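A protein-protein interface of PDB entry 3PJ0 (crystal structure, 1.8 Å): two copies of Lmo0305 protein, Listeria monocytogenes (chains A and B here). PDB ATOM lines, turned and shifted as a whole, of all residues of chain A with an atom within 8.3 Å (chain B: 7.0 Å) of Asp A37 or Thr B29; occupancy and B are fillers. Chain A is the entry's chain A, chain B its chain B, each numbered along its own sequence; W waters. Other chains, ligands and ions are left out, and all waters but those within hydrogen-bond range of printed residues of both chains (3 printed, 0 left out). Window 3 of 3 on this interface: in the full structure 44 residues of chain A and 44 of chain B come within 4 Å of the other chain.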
ATOM      1  N   LEU A  28     -14.940  25.348  10.736  1.00  0.00           N
ATOM      2  CA  LEU A  28     -14.069  25.435  11.921  1.00  0.00           C
ATOM      3  C   LEU A  28     -14.546  26.513  12.901  1.00  0.00           C
ATOM      4  O   LEU A  28     -14.621  26.287  14.110  1.00  0.00           O
ATOM      5  CB  LEU A  28     -12.616  25.710  11.485  1.00  0.00           C
ATOM      6  CG  LEU A  28     -11.546  25.825  12.608  1.00  0.00           C
ATOM      7  CD1 LEU A  28     -11.584  24.630  13.578  1.00  0.00           C
ATOM      8  CD2 LEU A  28     -10.178  26.028  12.020  1.00  0.00           C
ATOM      9  N   THR A  29     -14.846  27.702  12.398  1.00  0.00           N
ATOM     10  CA  THR A  29     -15.268  28.795  13.294  1.00  0.00           C
ATOM     11  C   THR A  29     -16.558  28.393  14.042  1.00  0.00           C
ATOM     12  O   THR A  29     -16.681  28.658  15.246  1.00  0.00           O
ATOM     13  CB  THR A  29     -15.398  30.158  12.570  1.00  0.00           C
ATOM     14  OG1 THR A  29     -16.420  30.088  11.589  1.00  0.00           O
ATOM     15  CG2 THR A  29     -14.064  30.590  11.920  1.00  0.00           C
ATOM     16  N   LEU A  32     -15.715  26.279  16.988  1.00  0.00           N
ATOM     17  CA  LEU A  32     -15.021  26.999  18.072  1.00  0.00           C
ATOM     18  C   LEU A  32     -15.912  27.960  18.851  1.00  0.00           C
ATOM     19  O   LEU A  32     -15.456  28.581  19.803  1.00  0.00           O
ATOM     20  CB  LEU A  32     -13.829  27.767  17.535  1.00  0.00           C
ATOM     21  CG  LEU A  32     -12.701  26.920  16.950  1.00  0.00           C
ATOM     22  CD1 LEU A  32     -11.595  27.870  16.423  1.00  0.00           C
ATOM     23  CD2 LEU A  32     -12.186  25.946  17.990  1.00  0.00           C
ATOM     24  N   GLN A  33     -17.188  28.064  18.471  1.00  0.00           N
ATOM     25  CA  GLN A  33     -18.073  29.037  19.124  1.00  0.00           C
ATOM     26  C   GLN A  33     -18.161  28.840  20.617  1.00  0.00           C
ATOM     27  O   GLN A  33     -18.141  29.822  21.366  1.00  0.00           O
ATOM     28  CB  GLN A  33     -19.478  29.014  18.496  1.00  0.00           C
ATOM     29  CG  GLN A  33     -19.464  29.622  17.086  1.00  0.00           C
ATOM     30  CD  GLN A  33     -20.807  29.666  16.425  1.00  0.00           C
ATOM     31  OE1 GLN A  33     -21.677  28.835  16.686  1.00  0.00           O
ATOM     32  NE2 GLN A  33     -20.965  30.627  15.479  1.00  0.00           N
ATOM     33  N   ASN A  34     -18.317  27.587  21.044  1.00  0.00           N
ATOM     34  CA  ASN A  34     -18.491  27.303  22.480  1.00  0.00           C
ATOM     35  C   ASN A  34     -17.205  27.001  23.251  1.00  0.00           C
ATOM     36  O   ASN A  34     -17.266  26.650  24.425  1.00  0.00           O
ATOM     37  CB  ASN A  34     -19.506  26.166  22.707  1.00  0.00           C
ATOM     38  CG  ASN A  34     -18.969  24.791  22.283  1.00  0.00           C
ATOM     39  OD1 ASN A  34     -17.931  24.691  21.661  1.00  0.00           O
ATOM     40  ND2 ASN A  34     -19.709  23.722  22.623  1.00  0.00           N
ATOM     41  N   ILE A  35     -16.059  27.167  22.603  1.00  0.00           N
ATOM     42  CA  ILE A  35     -14.751  26.843  23.185  1.00  0.00           C
ATOM     43  C   ILE A  35     -14.090  28.097  23.772  1.00  0.00           C
ATOM     44  O   ILE A  35     -14.052  29.145  23.147  1.00  0.00           O
ATOM     45  CB  ILE A  35     -13.814  26.216  22.151  1.00  0.00           C
ATOM     46  CG1 ILE A  35     -14.431  24.963  21.527  1.00  0.00           C
ATOM     47  CG2 ILE A  35     -12.428  25.935  22.789  1.00  0.00           C
ATOM     48  CD1 ILE A  35     -14.610  23.756  22.495  1.00  0.00           C
ATOM     49  N   ASP A  36     -13.571  27.966  24.986  1.00  0.00           N
ATOM     50  CA  ASP A  36     -12.900  29.059  25.689  1.00  0.00           C
ATOM     51  C   ASP A  36     -11.516  29.304  25.069  1.00  0.00           C
ATOM     52  O   ASP A  36     -10.754  28.359  24.858  1.00  0.00           O
ATOM     53  CB  ASP A  36     -12.770  28.660  27.167  1.00  0.00           C
ATOM     54  CG  ASP A  36     -12.277  29.778  28.065  1.00  0.00           C
ATOM     55  OD1 ASP A  36     -11.638  30.761  27.633  1.00  0.00           O
ATOM     56  OD2 ASP A  36     -12.534  29.644  29.287  1.00  0.00           O
ATOM     57  N   ASP A  37     -11.214  30.554  24.713  1.00  0.00           N
ATOM     58  CA  ASP A  37      -9.895  30.865  24.132  1.00  0.00           C
ATOM     59  C   ASP A  37      -8.733  30.483  25.055  1.00  0.00           C
ATOM     60  O   ASP A  37      -7.597  30.305  24.587  1.00  0.00           O
ATOM     61  CB  ASP A  37      -9.790  32.354  23.765  1.00  0.00           C
ATOM     62  CG  ASP A  37     -10.582  32.714  22.508  1.00  0.00           C
ATOM     63  OD1 ASP A  37     -10.757  31.866  21.608  1.00  0.00           O
ATOM     64  OD2 ASP A  37     -11.031  33.878  22.426  1.00  0.00           O
ATOM     65  N   ASN A  38      -9.002  30.383  26.356  1.00  0.00           N
ATOM     66  CA  ASN A  38      -7.978  29.994  27.328  1.00  0.00           C
ATOM     67  C   ASN A  38      -7.778  28.501  27.459  1.00  0.00           C
ATOM     68  O   ASN A  38      -6.924  28.083  28.239  1.00  0.00           O
ATOM     69  CB  ASN A  38      -8.287  30.597  28.703  1.00  0.00           C
ATOM     70  CG  ASN A  38      -8.181  32.107  28.705  1.00  0.00           C
ATOM     71  OD1 ASN A  38      -7.289  32.680  28.060  1.00  0.00           O
ATOM     72  ND2 ASN A  38      -9.099  32.769  29.417  1.00  0.00           N
ATOM     73  N   LEU A  39      -8.535  27.693  26.700  1.00  0.00           N
ATOM     74  CA  LEU A  39      -8.372  26.248  26.748  1.00  0.00           C
ATOM     75  C   LEU A  39      -6.984  25.899  26.253  1.00  0.00           C
ATOM     76  O   LEU A  39      -6.586  26.333  25.170  1.00  0.00           O
ATOM     77  CB  LEU A  39      -9.417  25.516  25.891  1.00  0.00           C
ATOM     78  CG  LEU A  39      -9.278  24.012  25.782  1.00  0.00           C
ATOM     79  CD1 LEU A  39      -9.342  23.331  27.183  1.00  0.00           C
ATOM     80  CD2 LEU A  39     -10.346  23.469  24.798  1.00  0.00           C
ATOM     81  N   GLU A  40      -6.256  25.110  27.044  1.00  0.00           N
ATOM     82  CA  GLU A  40      -4.901  24.779  26.690  1.00  0.00           C
ATOM     83  C   GLU A  40      -4.839  23.742  25.580  1.00  0.00           C
ATOM     84  O   GLU A  40      -5.589  22.788  25.547  1.00  0.00           O
ATOM     85  CB  GLU A  40      -4.103  24.291  27.902  1.00  0.00           C
ATOM     86  CG  GLU A  40      -3.761  25.386  28.924  1.00  0.00           C
ATOM     87  CD  GLU A  40      -2.605  26.287  28.503  1.00  0.00           C
ATOM     88  OE1 GLU A  40      -1.672  25.825  27.801  1.00  0.00           O
ATOM     89  OE2 GLU A  40      -2.602  27.471  28.900  1.00  0.00           O
ATOM     90  N   SER A  41      -3.879  23.950  24.695  1.00  0.00           N
ATOM     91  CA  SER A  41      -3.600  23.016  23.660  1.00  0.00           C
ATOM     92  C   SER A  41      -3.065  21.712  24.242  1.00  0.00           C
ATOM     93  O   SER A  41      -2.391  21.692  25.293  1.00  0.00           O
ATOM     94  CB  SER A  41      -2.512  23.571  22.719  1.00  0.00           C
ATOM     95  OG  SER A  41      -2.145  22.587  21.743  1.00  0.00           O
ATOM     96  N   TYR A 243      -5.399  19.875  18.496  1.00  0.00           N
ATOM     97  CA  TYR A 243      -6.722  20.381  18.892  1.00  0.00           C
ATOM     98  C   TYR A 243      -7.620  20.966  17.762  1.00  0.00           C
ATOM     99  O   TYR A 243      -8.840  20.826  17.872  1.00  0.00           O
ATOM    100  CB  TYR A 243      -6.654  21.375  20.069  1.00  0.00           C
ATOM    101  CG  TYR A 243      -6.094  22.719  19.722  1.00  0.00           C
ATOM    102  CD1 TYR A 243      -6.905  23.711  19.170  1.00  0.00           C
ATOM    103  CD2 TYR A 243      -4.751  23.023  19.952  1.00  0.00           C
ATOM    104  CE1 TYR A 243      -6.369  24.962  18.843  1.00  0.00           C
ATOM    105  CE2 TYR A 243      -4.234  24.266  19.643  1.00  0.00           C
ATOM    106  CZ  TYR A 243      -5.035  25.224  19.092  1.00  0.00           C
ATOM    107  OH  TYR A 243      -4.532  26.460  18.777  1.00  0.00           O
ATOM    108  N   ARG B  23       0.093  28.484  24.677  1.00  0.00           N
ATOM    109  CA  ARG B  23      -0.391  27.739  23.507  1.00  0.00           C
ATOM    110  C   ARG B  23      -1.807  27.316  23.867  1.00  0.00           C
ATOM    111  O   ARG B  23      -2.027  26.270  24.487  1.00  0.00           O
ATOM    112  CB  ARG B  23       0.473  26.500  23.204  1.00  0.00           C
ATOM    113  CG  ARG B  23       1.868  26.843  22.728  1.00  0.00           C
ATOM    114  CD  ARG B  23       2.674  25.597  22.296  1.00  0.00           C
ATOM    115  NE  ARG B  23       4.018  25.976  21.873  1.00  0.00           N
ATOM    116  CZ  ARG B  23       4.393  26.298  20.629  1.00  0.00           C
ATOM    117  NH1 ARG B  23       3.532  26.294  19.611  1.00  0.00           N
ATOM    118  NH2 ARG B  23       5.668  26.629  20.399  1.00  0.00           N
ATOM    119  N   ASN B  24      -2.761  28.181  23.550  1.00  0.00           N
ATOM    120  CA  ASN B  24      -4.170  27.925  23.825  1.00  0.00           C
ATOM    121  C   ASN B  24      -5.019  28.147  22.555  1.00  0.00           C
ATOM    122  O   ASN B  24      -4.504  28.542  21.506  1.00  0.00           O
ATOM    123  CB  ASN B  24      -4.659  28.761  25.014  1.00  0.00           C
ATOM    124  CG  ASN B  24      -4.507  30.270  24.780  1.00  0.00           C
ATOM    125  OD1 ASN B  24      -4.535  30.748  23.636  1.00  0.00           O
ATOM    126  ND2 ASN B  24      -4.371  31.034  25.881  1.00  0.00           N
ATOM    127  N   VAL B  25      -6.306  27.816  22.641  1.00  0.00           N
ATOM    128  CA  VAL B  25      -7.205  27.922  21.492  1.00  0.00           C
ATOM    129  C   VAL B  25      -7.244  29.340  20.918  1.00  0.00           C
ATOM    130  O   VAL B  25      -7.364  29.533  19.708  1.00  0.00           O
ATOM    131  CB  VAL B  25      -8.607  27.347  21.850  1.00  0.00           C
ATOM    132  CG1 VAL B  25      -9.626  27.640  20.755  1.00  0.00           C
ATOM    133  CG2 VAL B  25      -8.486  25.857  22.088  1.00  0.00           C
ATOM    134  N   GLY B  26      -7.090  30.327  21.794  1.00  0.00           N
ATOM    135  CA  GLY B  26      -6.968  31.729  21.397  1.00  0.00           C
ATOM    136  C   GLY B  26      -5.963  32.001  20.308  1.00  0.00           C
ATOM    137  O   GLY B  26      -6.140  32.953  19.524  1.00  0.00           O
ATOM    138  N   VAL B  27      -4.874  31.223  20.266  1.00  0.00           N
ATOM    139  CA  VAL B  27      -3.883  31.387  19.209  1.00  0.00           C
ATOM    140  C   VAL B  27      -4.571  31.179  17.835  1.00  0.00           C
ATOM    141  O   VAL B  27      -4.336  31.907  16.874  1.00  0.00           O
ATOM    142  CB  VAL B  27      -2.682  30.393  19.392  1.00  0.00           C
ATOM    143  CG1 VAL B  27      -1.711  30.455  18.190  1.00  0.00           C
ATOM    144  CG2 VAL B  27      -1.935  30.659  20.716  1.00  0.00           C
ATOM    145  N   LEU B  28      -5.398  30.151  17.741  1.00  0.00           N
ATOM    146  CA  LEU B  28      -6.148  29.875  16.524  1.00  0.00           C
ATOM    147  C   LEU B  28      -7.218  30.929  16.294  1.00  0.00           C
ATOM    148  O   LEU B  28      -7.382  31.410  15.162  1.00  0.00           O
ATOM    149  CB  LEU B  28      -6.776  28.480  16.586  1.00  0.00           C
ATOM    150  CG  LEU B  28      -7.603  27.982  15.393  1.00  0.00           C
ATOM    151  CD1 LEU B  28      -6.837  27.996  14.045  1.00  0.00           C
ATOM    152  CD2 LEU B  28      -8.096  26.584  15.666  1.00  0.00           C
ATOM    153  N   THR B  29      -7.961  31.268  17.342  1.00  0.00           N
ATOM    154  CA  THR B  29      -9.040  32.274  17.214  1.00  0.00           C
ATOM    155  C   THR B  29      -8.510  33.561  16.574  1.00  0.00           C
ATOM    156  O   THR B  29      -9.095  34.076  15.609  1.00  0.00           O
ATOM    157  CB  THR B  29      -9.682  32.599  18.584  1.00  0.00           C
ATOM    158  OG1 THR B  29     -10.331  31.429  19.083  1.00  0.00           O
ATOM    159  CG2 THR B  29     -10.735  33.735  18.457  1.00  0.00           C
ATOM    160  N   GLU B  30      -7.407  34.073  17.116  1.00  0.00           N
ATOM    161  CA  GLU B  30      -6.807  35.319  16.624  1.00  0.00           C
ATOM    162  C   GLU B  30      -6.415  35.223  15.140  1.00  0.00           C
ATOM    163  O   GLU B  30      -6.618  36.161  14.374  1.00  0.00           O
ATOM    164  CB  GLU B  30      -5.582  35.703  17.473  1.00  0.00           C
ATOM    165  CG  GLU B  30      -4.811  36.922  16.927  1.00  0.00           C
ATOM    166  CD  GLU B  30      -3.598  37.316  17.752  1.00  0.00           C
ATOM    167  OE1 GLU B  30      -3.473  36.910  18.941  1.00  0.00           O
ATOM    168  OE2 GLU B  30      -2.743  38.033  17.190  1.00  0.00           O
ATOM    169  N   ALA B  31      -5.875  34.077  14.736  1.00  0.00           N
ATOM    170  CA  ALA B  31      -5.435  33.888  13.362  1.00  0.00           C
ATOM    171  C   ALA B  31      -6.572  33.891  12.365  1.00  0.00           C
ATOM    172  O   ALA B  31      -6.355  34.227  11.188  1.00  0.00           O
ATOM    173  CB  ALA B  31      -4.609  32.573  13.231  1.00  0.00           C
ATOM    174  N   LEU B  32      -7.770  33.531  12.823  1.00  0.00           N
ATOM    175  CA  LEU B  32      -8.955  33.445  11.947  1.00  0.00           C
ATOM    176  C   LEU B  32      -9.856  34.671  11.922  1.00  0.00           C
ATOM    177  O   LEU B  32     -10.782  34.722  11.104  1.00  0.00           O
ATOM    178  CB  LEU B  32      -9.811  32.245  12.376  1.00  0.00           C
ATOM    179  CG  LEU B  32      -9.128  30.873  12.301  1.00  0.00           C
ATOM    180  CD1 LEU B  32     -10.062  29.752  12.743  1.00  0.00           C
ATOM    181  CD2 LEU B  32      -8.665  30.622  10.871  1.00  0.00           C
ATOM    182  N   GLN B  33      -9.558  35.694  12.722  1.00  0.00           N
ATOM    183  CA  GLN B  33     -10.469  36.835  12.877  1.00  0.00           C
ATOM    184  C   GLN B  33     -10.737  37.584  11.590  1.00  0.00           C
ATOM    185  O   GLN B  33     -11.864  38.066  11.388  1.00  0.00           O
ATOM    186  CB  GLN B  33      -9.990  37.823  13.964  1.00  0.00           C
ATOM    187  CG  GLN B  33     -10.105  37.287  15.370  1.00  0.00           C
ATOM    188  CD  GLN B  33      -9.810  38.324  16.437  1.00  0.00           C
ATOM    189  OE1 GLN B  33      -8.676  38.783  16.577  1.00  0.00           O
ATOM    190  NE2 GLN B  33     -10.840  38.687  17.216  1.00  0.00           N
ATOM    191  N   ASN B  34      -9.733  37.661  10.726  1.00  0.00           N
ATOM    192  CA  ASN B  34      -9.886  38.368   9.454  1.00  0.00           C
ATOM    193  C   ASN B  34     -10.033  37.477   8.216  1.00  0.00           C
ATOM    194  O   ASN B  34      -9.898  37.951   7.079  1.00  0.00           O
ATOM    195  CB  ASN B  34      -8.753  39.378   9.320  1.00  0.00           C
ATOM    196  CG  ASN B  34      -8.899  40.525  10.350  1.00  0.00           C
ATOM    197  OD1 ASN B  34      -8.101  40.619  11.269  1.00  0.00           O
ATOM    198  ND2 ASN B  34      -9.984  41.294  10.259  1.00  0.00           N
ATOM    199  N   ILE B 213       0.898  27.273  15.282  1.00  0.00           N
ATOM    200  CA  ILE B 213       0.331  26.109  15.957  1.00  0.00           C
ATOM    201  C   ILE B 213       1.109  24.847  15.612  1.00  0.00           C
ATOM    202  O   ILE B 213       1.581  24.143  16.509  1.00  0.00           O
ATOM    203  CB  ILE B 213      -1.186  25.976  15.645  1.00  0.00           C
ATOM    204  CG1 ILE B 213      -1.906  27.270  16.071  1.00  0.00           C
ATOM    205  CG2 ILE B 213      -1.799  24.759  16.372  1.00  0.00           C
ATOM    206  CD1 ILE B 213      -3.381  27.314  15.648  1.00  0.00           C
ATOM    207  N   TYR B 252       0.931  34.076  11.867  1.00  0.00           N
ATOM    208  CA  TYR B 252       2.025  34.301  12.811  1.00  0.00           C
ATOM    209  C   TYR B 252       3.363  34.590  12.122  1.00  0.00           C
ATOM    210  O   TYR B 252       4.182  35.319  12.662  1.00  0.00           O
ATOM    211  CB  TYR B 252       2.077  33.163  13.834  1.00  0.00           C
ATOM    212  CG  TYR B 252       0.872  33.271  14.743  1.00  0.00           C
ATOM    213  CD1 TYR B 252       0.782  34.316  15.668  1.00  0.00           C
ATOM    214  CD2 TYR B 252      -0.207  32.390  14.649  1.00  0.00           C
ATOM    215  CE1 TYR B 252      -0.345  34.484  16.461  1.00  0.00           C
ATOM    216  CE2 TYR B 252      -1.348  32.540  15.461  1.00  0.00           C
ATOM    217  CZ  TYR B 252      -1.407  33.588  16.359  1.00  0.00           C
ATOM    218  OH  TYR B 252      -2.521  33.746  17.145  1.00  0.00           O
HETATM  219  O   HOH W   1      -4.433  29.399  28.473  1.00  0.00           O
HETATM  220  O   HOH W   2      -2.488  26.933  20.372  1.00  0.00           O
HETATM  221  O   HOH W   3       0.653  27.070  27.135  1.00  0.00           O
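Leu A28 touches Leu B32.
Leu A32 touches Leu B28 (CD1 to CD2, 3.8 Å).
CG1 of Val B25 touches CG2 of Ile A35, 3.9 Å away.
Val B25 touches Asp A36 (CB to O, 3.8 Å).
C of Asn A38 touches CB of Asn B24, 3.97 Å away.
Asn B24 touches Leu A39 (CB to O, 3.1 Å).
CD1 of Tyr A243 touches CG2 of Val B25, 3.95 Å away.
Tyr A243 touches Leu B28.
Ile B213 touches Tyr A243.
Water W2 lies within hydrogen-bond range of OH of Tyr A243 (2.6 Å) and O of Asn B24 (2.8 Å).
Water W1 lies within hydrogen-bond range of the side-chain carboxylate (OE2) of Glu A40, the backbone carbonyl oxygen (O) of Asn A38 and the side-chain amide nitrogen (ND2) of Asn B24.
Water W3 lies within hydrogen-bond range of OE1 of Glu A40 (2.7 Å) and N of Arg B23 (2.9 Å).
Of the 13 printed residues of chain A, 10 touch a printed residue of chain B.
Hydrophobic or aromatic side chains of chain A that line the printed part of chain B: Leu A28, Leu A32, Ile A35, Leu A39 and Tyr A243.
Among the printed residues, 17 pairs touch across the chains.
Among the printed residues, no Asp or Glu carboxylate lies within 4 Å of a Lys or Arg side-chain nitrogen of the other chain.
Leu A28 touches Leu B32, and with the chains exchanged Leu A32 touches Leu B28.
The side-chain amide oxygen of Asn B24 sits close to the backbone NH of Gly B26 (3.2 Å).
OD1 of Asp A36 sits at hydrogen-bond distance from N of Asn A38, 3.0 Å away.
The backbone NH of Val B27 sits at hydrogen-bond distance from the side-chain amide oxygen of Asn B24 (3.4 Å).
Printed residues of chain A within 4 Å of Leu B28: Leu A32 (3.8 Å) and Tyr A243 (3.7 Å).
Printed residues of chain B within 4 Å of Leu A28: Leu B32 (3.8 Å).
Asn A34 touches none of the printed residues of chain B.
Gln A33 touches none of the printed residues of chain B.
The nearest residue of chain B that does not touch Asp A37 is Val B27 (5.2 Å).
The nearest printed residue of chain B that does not touch Asn A38 is Gly B26 (4.9 Å).
O of Arg B23 is in hydrogen-bond range of N of Ser A41, at 3.0 Å.
The side-chain carboxylate of Glu A40 lies close to the backbone carbonyl oxygen of Arg B23 (3.4 Å).
OH of Tyr A243 lies within hydrogen-bond range of O of Asn B24 (3.4 Å).
The backbone NH of Val B25 is in hydrogen-bond range of the backbone carbonyl oxygen of Leu A39.
The side-chain hydroxyl of Thr B29 lies within hydrogen-bond range of the side-chain carboxylate of Asp A37, at 2.6 Å.
N of Val B25 sits at hydrogen-bond distance from O of Asp A37 (3.4 Å).
The side-chain amide oxygen (OD1) of Asn B24 sits close to the backbone carbonyl oxygen (O) of Asp A37 (3.2 Å).
O of Asp A37 lies within hydrogen-bond range of N of Gly B26, at 2.8 Å.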
